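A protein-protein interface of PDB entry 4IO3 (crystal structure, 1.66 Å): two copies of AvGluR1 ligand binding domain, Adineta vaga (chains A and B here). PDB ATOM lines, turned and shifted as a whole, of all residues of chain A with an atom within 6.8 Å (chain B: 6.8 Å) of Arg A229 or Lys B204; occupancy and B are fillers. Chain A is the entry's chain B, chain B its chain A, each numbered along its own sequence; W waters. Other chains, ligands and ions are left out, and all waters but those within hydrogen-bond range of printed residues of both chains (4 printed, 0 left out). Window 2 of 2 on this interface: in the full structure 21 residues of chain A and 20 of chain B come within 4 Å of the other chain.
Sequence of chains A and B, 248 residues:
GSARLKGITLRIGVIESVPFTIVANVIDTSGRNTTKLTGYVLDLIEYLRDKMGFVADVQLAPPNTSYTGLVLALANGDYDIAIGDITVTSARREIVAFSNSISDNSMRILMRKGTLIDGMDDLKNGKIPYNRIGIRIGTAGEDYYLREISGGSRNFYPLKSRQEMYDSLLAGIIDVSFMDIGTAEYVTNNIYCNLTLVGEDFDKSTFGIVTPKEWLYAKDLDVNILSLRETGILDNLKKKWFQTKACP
The side-chain hydroxyl (OG1) of Thr B206 lies within hydrogen-bond range of the guanidinium group (NH1) of Arg A229 (3.1 Å).
The guanidinium group of Arg B147 lies within hydrogen-bond range of the backbone carbonyl oxygen of Glu A230 (2.9 Å).
N of Val B88 sits at hydrogen-bond distance from O of Thr B206.
O of Ser A101 is in hydrogen-bond range of NH2 of Arg A229 (2.8 Å).
NZ of Lys B204 is in salt-bridge range of OD1 of Asp B201, 3.0 Å away.
Val B88 touches Asn A100 (CG1 to ND2, 3.5 Å).
CD1 of Leu A226 touches CG1 of Val B88, at 3.7 Å.
Leu A226 touches Thr B89.
O of Lys B204 touches CD of Arg A229, 3.8 Å away.
Glu A230 touches Thr B89.
Lys B204 touches just one residue of chain A: Arg A229.
Of the printed residues of chain A, Thr B206 touches Arg A229.
Of the printed residues of chain A, Thr B89 touches Leu A226 and Glu A230.
Printed residues of chain A within 4 Å of Val B88: Asn A100 and Leu A226.
Printed residues of chain A within 4 Å of Arg B147: Glu A230.
Of the printed residues of chain B, Leu A226 touches Val B88 and Thr B89.
The nearest residue of chain B that does not touch Arg A229 is Ser B205 (4.1 Å).
The nearest printed residue of chain A that does not touch Val B88 is Glu A230 (4.4 Å).
Hydrophobic or aromatic side chains of chain B within 4 Å of the printed part of chain A: Val B88.
Along chain B the printed residues that touch a printed residue of chain A span positions 88 to 206.
Printed residues of chain A that touch a printed residue of chain B: Asn A100, Leu A226, Arg A229 and Glu A230.
Among the printed residues, no Asp or Glu carboxylate lies within 4 Å of a Lys or Arg side-chain nitrogen of the other chain.
No position is printed for both chains.
Water W2 lies within hydrogen-bond range of O of Val B88, NH1 of Arg A229 and N of Thr B206.
Water W3 lies within hydrogen-bond range of OD1 of Asp B203 (2.7 Å), O of Glu A230 (3.0 Å) and NH2 of Arg B147 (3.0 Å).
Water W4 lies within hydrogen-bond range of the backbone carbonyl oxygen of Lys B204 (2.8 Å) and the backbone carbonyl oxygen of Arg A229 (3.3 Å).
Water W1 lies within hydrogen-bond range of the backbone carbonyl oxygen of Val B88 (3.0 Å) and the side-chain carboxylate of Glu A230 (3.0 Å).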
ATOM      1  N   ASN A 100      14.258  18.909  30.213  1.00  0.00           N
ATOM      2  CA  ASN A 100      13.358  19.974  29.875  1.00  0.00           C
ATOM      3  C   ASN A 100      12.483  20.244  31.069  1.00  0.00           C
ATOM      4  O   ASN A 100      12.208  19.349  31.867  1.00  0.00           O
ATOM      5  CB  ASN A 100      12.532  19.596  28.657  1.00  0.00           C
ATOM      6  CG  ASN A 100      13.362  19.603  27.422  1.00  0.00           C
ATOM      7  OD1 ASN A 100      13.826  18.564  26.975  1.00  0.00           O
ATOM      8  ND2 ASN A 100      13.597  20.790  26.876  1.00  0.00           N
ATOM      9  N   SER A 101      12.060  21.483  31.207  1.00  0.00           N
ATOM     10  CA  SER A 101      11.344  21.875  32.401  1.00  0.00           C
ATOM     11  C   SER A 101       9.989  21.213  32.522  1.00  0.00           C
ATOM     12  O   SER A 101       9.232  21.095  31.546  1.00  0.00           O
ATOM     13  CB  SER A 101      11.181  23.373  32.461  1.00  0.00           C
ATOM     14  OG  SER A 101      10.563  23.844  31.290  1.00  0.00           O
ATOM     15  N   ILE A 102       9.694  20.794  33.747  1.00  0.00           N
ATOM     16  CA  ILE A 102       8.413  20.195  34.078  1.00  0.00           C
ATOM     17  C   ILE A 102       7.399  21.243  34.516  1.00  0.00           C
ATOM     18  O   ILE A 102       6.202  20.986  34.540  1.00  0.00           O
ATOM     19  CB  ILE A 102       8.504  19.078  35.151  1.00  0.00           C
ATOM     20  CG1 ILE A 102       9.066  19.599  36.455  1.00  0.00           C
ATOM     21  CG2 ILE A 102       9.336  17.894  34.659  1.00  0.00           C
ATOM     22  CD1 ILE A 102       9.016  18.594  37.584  1.00  0.00           C
ATOM     23  N   SER A 103       7.852  22.462  34.820  1.00  0.00           N
ATOM     24  CA  SER A 103       6.955  23.492  35.306  1.00  0.00           C
ATOM     25  C   SER A 103       7.680  24.813  35.296  1.00  0.00           C
ATOM     26  O   SER A 103       8.904  24.868  35.515  1.00  0.00           O
ATOM     27  CB  SER A 103       6.519  23.180  36.751  1.00  0.00           C
ATOM     28  OG  SER A 103       5.698  24.204  37.311  1.00  0.00           O
ATOM     29  N   ASP A 104       6.943  25.883  35.053  1.00  0.00           N
ATOM     30  CA  ASP A 104       7.508  27.177  35.376  1.00  0.00           C
ATOM     31  C   ASP A 104       7.431  27.411  36.880  1.00  0.00           C
ATOM     32  O   ASP A 104       6.830  26.631  37.631  1.00  0.00           O
ATOM     33  CB  ASP A 104       6.858  28.305  34.580  1.00  0.00           C
ATOM     34  CG  ASP A 104       5.377  28.313  34.686  1.00  0.00           C
ATOM     35  OD1 ASP A 104       4.842  27.708  35.639  1.00  0.00           O
ATOM     36  OD2 ASP A 104       4.746  28.948  33.823  1.00  0.00           O
ATOM     37  N   ASN A 224      10.159  12.299  26.382  1.00  0.00           N
ATOM     38  CA  ASN A 224       9.006  11.924  27.171  1.00  0.00           C
ATOM     39  C   ASN A 224       8.398  13.075  27.990  1.00  0.00           C
ATOM     40  O   ASN A 224       7.180  13.223  28.051  1.00  0.00           O
ATOM     41  CB  ASN A 224       9.346  10.692  28.025  1.00  0.00           C
ATOM     42  CG  ASN A 224       9.217   9.402  27.241  1.00  0.00           C
ATOM     43  OD1 ASN A 224       8.124   8.847  27.128  1.00  0.00           O
ATOM     44  ND2 ASN A 224      10.315   8.945  26.649  1.00  0.00           N
ATOM     45  N   ILE A 225       9.234  13.895  28.615  1.00  0.00           N
ATOM     46  CA  ILE A 225       8.731  15.045  29.344  1.00  0.00           C
ATOM     47  C   ILE A 225       8.006  16.002  28.398  1.00  0.00           C
ATOM     48  O   ILE A 225       6.916  16.491  28.700  1.00  0.00           O
ATOM     49  CB  ILE A 225       9.860  15.781  30.094  1.00  0.00           C
ATOM     50  CG1 ILE A 225      10.429  14.897  31.207  1.00  0.00           C
ATOM     51  CG2 ILE A 225       9.373  17.065  30.674  1.00  0.00           C
ATOM     52  CD1 ILE A 225       9.415  14.525  32.279  1.00  0.00           C
ATOM     53  N   LEU A 226       8.590  16.249  27.233  1.00  0.00           N
ATOM     54  CA  LEU A 226       7.970  17.155  26.284  1.00  0.00           C
ATOM     55  C   LEU A 226       6.657  16.587  25.794  1.00  0.00           C
ATOM     56  O   LEU A 226       5.713  17.312  25.551  1.00  0.00           O
ATOM     57  CB  LEU A 226       8.909  17.435  25.115  1.00  0.00           C
ATOM     58  CG  LEU A 226      10.120  18.279  25.529  1.00  0.00           C
ATOM     59  CD1 LEU A 226      11.202  18.347  24.495  1.00  0.00           C
ATOM     60  CD2 LEU A 226       9.662  19.687  25.906  1.00  0.00           C
ATOM     61  N   SER A 227       6.597  15.276  25.643  1.00  0.00           N
ATOM     62  CA  SER A 227       5.350  14.660  25.215  1.00  0.00           C
ATOM     63  C   SER A 227       4.271  14.842  26.292  1.00  0.00           C
ATOM     64  O   SER A 227       3.116  15.160  25.998  1.00  0.00           O
ATOM     65  CB  SER A 227       5.582  13.188  24.917  1.00  0.00           C
ATOM     66  OG  SER A 227       4.346  12.552  24.632  1.00  0.00           O
ATOM     67  N   LEU A 228       4.638  14.629  27.547  1.00  0.00           N
ATOM     68  CA  LEU A 228       3.684  14.857  28.642  1.00  0.00           C
ATOM     69  C   LEU A 228       3.237  16.329  28.689  1.00  0.00           C
ATOM     70  O   LEU A 228       2.095  16.605  29.010  1.00  0.00           O
ATOM     71  CB  LEU A 228       4.270  14.448  29.993  1.00  0.00           C
ATOM     72  CG  LEU A 228       4.565  12.961  30.152  1.00  0.00           C
ATOM     73  CD1 LEU A 228       5.191  12.717  31.501  1.00  0.00           C
ATOM     74  CD2 LEU A 228       3.337  12.111  30.005  1.00  0.00           C
ATOM     75  N   ARG A 229       4.142  17.271  28.402  1.00  0.00           N
ATOM     76  CA  ARG A 229       3.771  18.684  28.326  1.00  0.00           C
ATOM     77  C   ARG A 229       2.730  18.891  27.232  1.00  0.00           C
ATOM     78  O   ARG A 229       1.665  19.472  27.464  1.00  0.00           O
ATOM     79  CB  ARG A 229       5.017  19.549  28.060  1.00  0.00           C
ATOM     80  CG  ARG A 229       4.807  21.025  27.780  1.00  0.00           C
ATOM     81  CD  ARG A 229       6.108  21.665  27.164  1.00  0.00           C
ATOM     82  NE  ARG A 229       7.204  21.705  28.150  1.00  0.00           N
ATOM     83  CZ  ARG A 229       8.375  22.349  28.000  1.00  0.00           C
ATOM     84  NH1 ARG A 229       8.674  23.024  26.893  1.00  0.00           N
ATOM     85  NH2 ARG A 229       9.261  22.318  28.978  1.00  0.00           N
ATOM     86  N   GLU A 230       3.046  18.406  26.033  1.00  0.00           N
ATOM     87  CA  GLU A 230       2.265  18.724  24.841  1.00  0.00           C
ATOM     88  C   GLU A 230       0.864  18.163  24.918  1.00  0.00           C
ATOM     89  O   GLU A 230      -0.083  18.783  24.440  1.00  0.00           O
ATOM     90  CB  GLU A 230       2.980  18.183  23.593  1.00  0.00           C
ATOM     91  CG  GLU A 230       4.196  19.018  23.277  1.00  0.00           C
ATOM     92  CD  GLU A 230       5.167  18.362  22.333  1.00  0.00           C
ATOM     93  OE1 GLU A 230       4.828  17.369  21.692  1.00  0.00           O
ATOM     94  OE2 GLU A 230       6.294  18.856  22.230  1.00  0.00           O
ATOM     95  N   THR A 231       0.749  16.990  25.517  1.00  0.00           N
ATOM     96  CA  THR A 231      -0.526  16.320  25.630  1.00  0.00           C
ATOM     97  C   THR A 231      -1.330  16.694  26.875  1.00  0.00           C
ATOM     98  O   THR A 231      -2.410  16.150  27.091  1.00  0.00           O
ATOM     99  CB  THR A 231      -0.370  14.782  25.555  1.00  0.00           C
ATOM    100  OG1 THR A 231       0.365  14.274  26.677  1.00  0.00           O
ATOM    101  CG2 THR A 231       0.323  14.372  24.259  1.00  0.00           C
ATOM    102  N   GLY A 232      -0.847  17.632  27.679  1.00  0.00           N
ATOM    103  CA  GLY A 232      -1.649  18.144  28.778  1.00  0.00           C
ATOM    104  C   GLY A 232      -1.565  17.362  30.083  1.00  0.00           C
ATOM    105  O   GLY A 232      -2.199  17.717  31.067  1.00  0.00           O
ATOM    106  N   ILE A 233      -0.733  16.328  30.116  1.00  0.00           N
ATOM    107  CA  ILE A 233      -0.585  15.520  31.327  1.00  0.00           C
ATOM    108  C   ILE A 233      -0.008  16.320  32.515  1.00  0.00           C
ATOM    109  O   ILE A 233      -0.498  16.212  33.654  1.00  0.00           O
ATOM    110  CB  ILE A 233       0.288  14.277  31.066  1.00  0.00           C
ATOM    111  CG1 ILE A 233      -0.355  13.369  30.015  1.00  0.00           C
ATOM    112  CG2 ILE A 233       0.513  13.514  32.353  1.00  0.00           C
ATOM    113  CD1 ILE A 233      -1.771  12.995  30.344  1.00  0.00           C
ATOM    114  N   LEU A 234       1.037  17.094  32.267  1.00  0.00           N
ATOM    115  CA  LEU A 234       1.647  17.893  33.329  1.00  0.00           C
ATOM    116  C   LEU A 234       0.631  18.882  33.873  1.00  0.00           C
ATOM    117  O   LEU A 234       0.549  19.082  35.080  1.00  0.00           O
ATOM    118  CB  LEU A 234       2.926  18.605  32.855  1.00  0.00           C
ATOM    119  CG  LEU A 234       4.060  17.678  32.423  1.00  0.00           C
ATOM    120  CD1 LEU A 234       5.311  18.470  32.106  1.00  0.00           C
ATOM    121  CD2 LEU A 234       4.342  16.603  33.457  1.00  0.00           C
ATOM    122  N   ASP A 235      -0.174  19.470  32.998  1.00  0.00           N
ATOM    123  CA  ASP A 235      -1.224  20.397  33.461  1.00  0.00           C
ATOM    124  C   ASP A 235      -2.287  19.699  34.297  1.00  0.00           C
ATOM    125  O   ASP A 235      -2.773  20.237  35.301  1.00  0.00           O
ATOM    126  CB  ASP A 235      -1.909  21.062  32.284  1.00  0.00           C
ATOM    127  CG  ASP A 235      -1.109  22.181  31.696  1.00  0.00           C
ATOM    128  OD1 ASP A 235      -0.173  22.663  32.354  1.00  0.00           O
ATOM    129  OD2 ASP A 235      -1.436  22.587  30.569  1.00  0.00           O
ATOM    130  N   THR B  87      10.396  26.948  18.984  1.00  0.00           N
ATOM    131  CA  THR B  87       9.701  26.173  20.002  1.00  0.00           C
ATOM    132  C   THR B  87      10.341  24.813  20.265  1.00  0.00           C
ATOM    133  O   THR B  87      10.698  24.083  19.339  1.00  0.00           O
ATOM    134  CB  THR B  87       8.229  25.986  19.597  1.00  0.00           C
ATOM    135  OG1 THR B  87       7.662  27.279  19.375  1.00  0.00           O
ATOM    136  CG2 THR B  87       7.421  25.283  20.677  1.00  0.00           C
ATOM    137  N   VAL B  88      10.502  24.500  21.554  1.00  0.00           N
ATOM    138  CA  VAL B  88      11.040  23.195  21.979  1.00  0.00           C
ATOM    139  C   VAL B  88       9.904  22.193  21.897  1.00  0.00           C
ATOM    140  O   VAL B  88       8.888  22.343  22.562  1.00  0.00           O
ATOM    141  CB  VAL B  88      11.580  23.272  23.407  1.00  0.00           C
ATOM    142  CG1 VAL B  88      12.115  21.927  23.860  1.00  0.00           C
ATOM    143  CG2 VAL B  88      12.661  24.295  23.497  1.00  0.00           C
ATOM    144  N   THR B  89      10.038  21.206  21.029  1.00  0.00           N
ATOM    145  CA  THR B  89       9.025  20.185  20.913  1.00  0.00           C
ATOM    146  C   THR B  89       9.616  18.792  21.012  1.00  0.00           C
ATOM    147  O   THR B  89      10.781  18.593  20.746  1.00  0.00           O
ATOM    148  CB  THR B  89       8.261  20.237  19.578  1.00  0.00           C
ATOM    149  OG1 THR B  89       9.143  19.823  18.522  1.00  0.00           O
ATOM    150  CG2 THR B  89       7.754  21.674  19.274  1.00  0.00           C
ATOM    151  N   ASN B 105       6.614  30.482  26.280  1.00  0.00           N
ATOM    152  CA  ASN B 105       5.860  30.756  25.059  1.00  0.00           C
ATOM    153  C   ASN B 105       4.497  30.123  25.197  1.00  0.00           C
ATOM    154  O   ASN B 105       4.284  29.249  26.031  1.00  0.00           O
ATOM    155  CB  ASN B 105       6.573  30.201  23.809  1.00  0.00           C
ATOM    156  CG  ASN B 105       5.833  30.516  22.499  1.00  0.00           C
ATOM    157  OD1 ASN B 105       5.572  31.693  22.184  1.00  0.00           O
ATOM    158  ND2 ASN B 105       5.486  29.474  21.737  1.00  0.00           N
ATOM    159  N   SER B 106       3.567  30.623  24.406  1.00  0.00           N
ATOM    160  CA  SER B 106       2.275  29.990  24.223  1.00  0.00           C
ATOM    161  C   SER B 106       1.765  30.565  22.926  1.00  0.00           C
ATOM    162  O   SER B 106       2.361  31.514  22.391  1.00  0.00           O
ATOM    163  CB  SER B 106       1.311  30.321  25.368  1.00  0.00           C
ATOM    164  OG  SER B 106       1.181  31.730  25.549  1.00  0.00           O
ATOM    165  N   MET B 107       0.644  30.056  22.443  1.00  0.00           N
ATOM    166  CA  MET B 107       0.042  30.580  21.216  1.00  0.00           C
ATOM    167  C   MET B 107      -1.287  31.224  21.470  1.00  0.00           C
ATOM    168  O   MET B 107      -1.940  30.929  22.470  1.00  0.00           O
ATOM    169  CB  MET B 107      -0.129  29.486  20.151  1.00  0.00           C
ATOM    170  CG  MET B 107       1.207  28.970  19.615  1.00  0.00           C
ATOM    171  SD  MET B 107       1.052  27.861  18.203  1.00  0.00           S
ATOM    172  CE  MET B 107       0.573  26.343  19.049  1.00  0.00           C
ATOM    173  N   ARG B 147      -2.867  17.536  15.984  1.00  0.00           N
ATOM    174  CA  ARG B 147      -3.208  16.730  17.160  1.00  0.00           C
ATOM    175  C   ARG B 147      -4.548  17.073  17.779  1.00  0.00           C
ATOM    176  O   ARG B 147      -5.276  16.181  18.229  1.00  0.00           O
ATOM    177  CB  ARG B 147      -2.121  16.809  18.256  1.00  0.00           C
ATOM    178  CG  ARG B 147      -2.491  15.878  19.440  1.00  0.00           C
ATOM    179  CD  ARG B 147      -1.537  15.912  20.644  1.00  0.00           C
ATOM    180  NE  ARG B 147      -1.515  17.239  21.253  1.00  0.00           N
ATOM    181  CZ  ARG B 147      -0.562  18.129  21.046  1.00  0.00           C
ATOM    182  NH1 ARG B 147       0.473  17.831  20.273  1.00  0.00           N
ATOM    183  NH2 ARG B 147      -0.643  19.327  21.613  1.00  0.00           N
ATOM    184  N   GLU B 200      -8.188  32.063  25.131  1.00  0.00           N
ATOM    185  CA  GLU B 200      -7.141  31.749  26.088  1.00  0.00           C
ATOM    186  C   GLU B 200      -5.879  31.296  25.339  1.00  0.00           C
ATOM    187  O   GLU B 200      -5.957  30.739  24.233  1.00  0.00           O
ATOM    188  CB  GLU B 200      -7.609  30.652  27.043  1.00  0.00           C
ATOM    189  CG  GLU B 200      -8.772  31.094  27.946  1.00  0.00           C
ATOM    190  CD  GLU B 200      -9.361  29.956  28.769  1.00  0.00           C
ATOM    191  OE1 GLU B 200      -8.831  28.821  28.700  1.00  0.00           O
ATOM    192  OE2 GLU B 200     -10.361  30.202  29.488  1.00  0.00           O
ATOM    193  N   ASP B 201      -4.724  31.534  25.924  1.00  0.00           N
ATOM    194  CA  ASP B 201      -3.526  31.044  25.261  1.00  0.00           C
ATOM    195  C   ASP B 201      -3.486  29.528  25.394  1.00  0.00           C
ATOM    196  O   ASP B 201      -4.132  28.950  26.267  1.00  0.00           O
ATOM    197  CB  ASP B 201      -2.241  31.714  25.749  1.00  0.00           C
ATOM    198  CG  ASP B 201      -2.028  31.575  27.217  1.00  0.00           C
ATOM    199  OD1 ASP B 201      -2.672  30.691  27.828  1.00  0.00           O
ATOM    200  OD2 ASP B 201      -1.205  32.353  27.757  1.00  0.00           O
ATOM    201  N   PHE B 202      -2.790  28.890  24.462  1.00  0.00           N
ATOM    202  CA  PHE B 202      -2.748  27.437  24.363  1.00  0.00           C
ATOM    203  C   PHE B 202      -1.340  26.988  23.967  1.00  0.00           C
ATOM    204  O   PHE B 202      -0.494  27.811  23.575  1.00  0.00           O
ATOM    205  CB  PHE B 202      -3.782  26.878  23.369  1.00  0.00           C
ATOM    206  CG  PHE B 202      -3.702  27.468  21.998  1.00  0.00           C
ATOM    207  CD1 PHE B 202      -4.284  28.699  21.726  1.00  0.00           C
ATOM    208  CD2 PHE B 202      -3.056  26.796  20.976  1.00  0.00           C
ATOM    209  CE1 PHE B 202      -4.212  29.245  20.442  1.00  0.00           C
ATOM    210  CE2 PHE B 202      -2.974  27.339  19.708  1.00  0.00           C
ATOM    211  CZ  PHE B 202      -3.553  28.557  19.442  1.00  0.00           C
ATOM    212  N   ASP B 203      -1.105  25.689  24.111  1.00  0.00           N
ATOM    213  CA  ASP B 203       0.184  25.077  23.817  1.00  0.00           C
ATOM    214  C   ASP B 203       1.343  25.754  24.541  1.00  0.00           C
ATOM    215  O   ASP B 203       2.306  26.200  23.914  1.00  0.00           O
ATOM    216  CB  ASP B 203       0.448  25.053  22.307  1.00  0.00           C
ATOM    217  CG  ASP B 203       1.496  24.030  21.928  1.00  0.00           C
ATOM    218  OD1 ASP B 203       1.518  22.953  22.558  1.00  0.00           O
ATOM    219  OD2 ASP B 203       2.292  24.294  20.999  1.00  0.00           O
ATOM    220  N   LYS B 204       1.242  25.854  25.856  1.00  0.00           N
ATOM    221  CA  LYS B 204       2.326  26.432  26.660  1.00  0.00           C
ATOM    222  C   LYS B 204       3.604  25.627  26.387  1.00  0.00           C
ATOM    223  O   LYS B 204       3.620  24.380  26.417  1.00  0.00           O
ATOM    224  CB  LYS B 204       1.987  26.374  28.140  1.00  0.00           C
ATOM    225  CG  LYS B 204       0.663  27.032  28.535  1.00  0.00           C
ATOM    226  CD  LYS B 204       0.707  28.555  28.435  1.00  0.00           C
ATOM    227  CE  LYS B 204      -0.269  29.235  29.414  1.00  0.00           C
ATOM    228  NZ  LYS B 204      -1.556  28.479  29.578  1.00  0.00           N
ATOM    229  N   SER B 205       4.687  26.357  26.141  1.00  0.00           N
ATOM    230  CA  SER B 205       5.893  25.770  25.664  1.00  0.00           C
ATOM    231  C   SER B 205       7.053  26.690  26.032  1.00  0.00           C
ATOM    232  O   SER B 205       6.881  27.656  26.805  1.00  0.00           O
ATOM    233  CB  SER B 205       5.790  25.614  24.144  1.00  0.00           C
ATOM    234  OG  SER B 205       5.291  26.817  23.533  1.00  0.00           O
ATOM    235  N   THR B 206       8.221  26.417  25.459  1.00  0.00           N
ATOM    236  CA  THR B 206       9.387  27.269  25.648  1.00  0.00           C
ATOM    237  C   THR B 206      10.119  27.481  24.350  1.00  0.00           C
ATOM    238  O   THR B 206       9.931  26.709  23.396  1.00  0.00           O
ATOM    239  CB  THR B 206      10.360  26.618  26.628  1.00  0.00           C
ATOM    240  OG1 THR B 206      10.677  25.290  26.179  1.00  0.00           O
ATOM    241  CG2 THR B 206       9.725  26.531  28.005  1.00  0.00           C
ATOM    242  N   PHE B 207      10.952  28.515  24.300  1.00  0.00           N
ATOM    243  CA  PHE B 207      11.903  28.696  23.219  1.00  0.00           C
ATOM    244  C   PHE B 207      13.277  28.316  23.764  1.00  0.00           C
ATOM    245  O   PHE B 207      13.620  28.685  24.890  1.00  0.00           O
ATOM    246  CB  PHE B 207      11.992  30.147  22.742  1.00  0.00           C
ATOM    247  CG  PHE B 207      10.751  30.682  22.086  1.00  0.00           C
ATOM    248  CD1 PHE B 207       9.912  29.865  21.360  1.00  0.00           C
ATOM    249  CD2 PHE B 207      10.490  32.035  22.125  1.00  0.00           C
ATOM    250  CE1 PHE B 207       8.794  30.388  20.747  1.00  0.00           C
ATOM    251  CE2 PHE B 207       9.372  32.580  21.517  1.00  0.00           C
ATOM    252  CZ  PHE B 207       8.543  31.763  20.802  1.00  0.00           C
HETATM  253  O   HOH W   1       5.925  21.810  22.784  1.00  0.00           O
HETATM  254  O   HOH W   2       7.792  23.625  24.454  1.00  0.00           O
HETATM  255  O   HOH W   3      -0.598  21.570  23.609  1.00  0.00           O
HETATM  256  O   HOH W   4       1.641  22.783  27.555  1.00  0.00           O
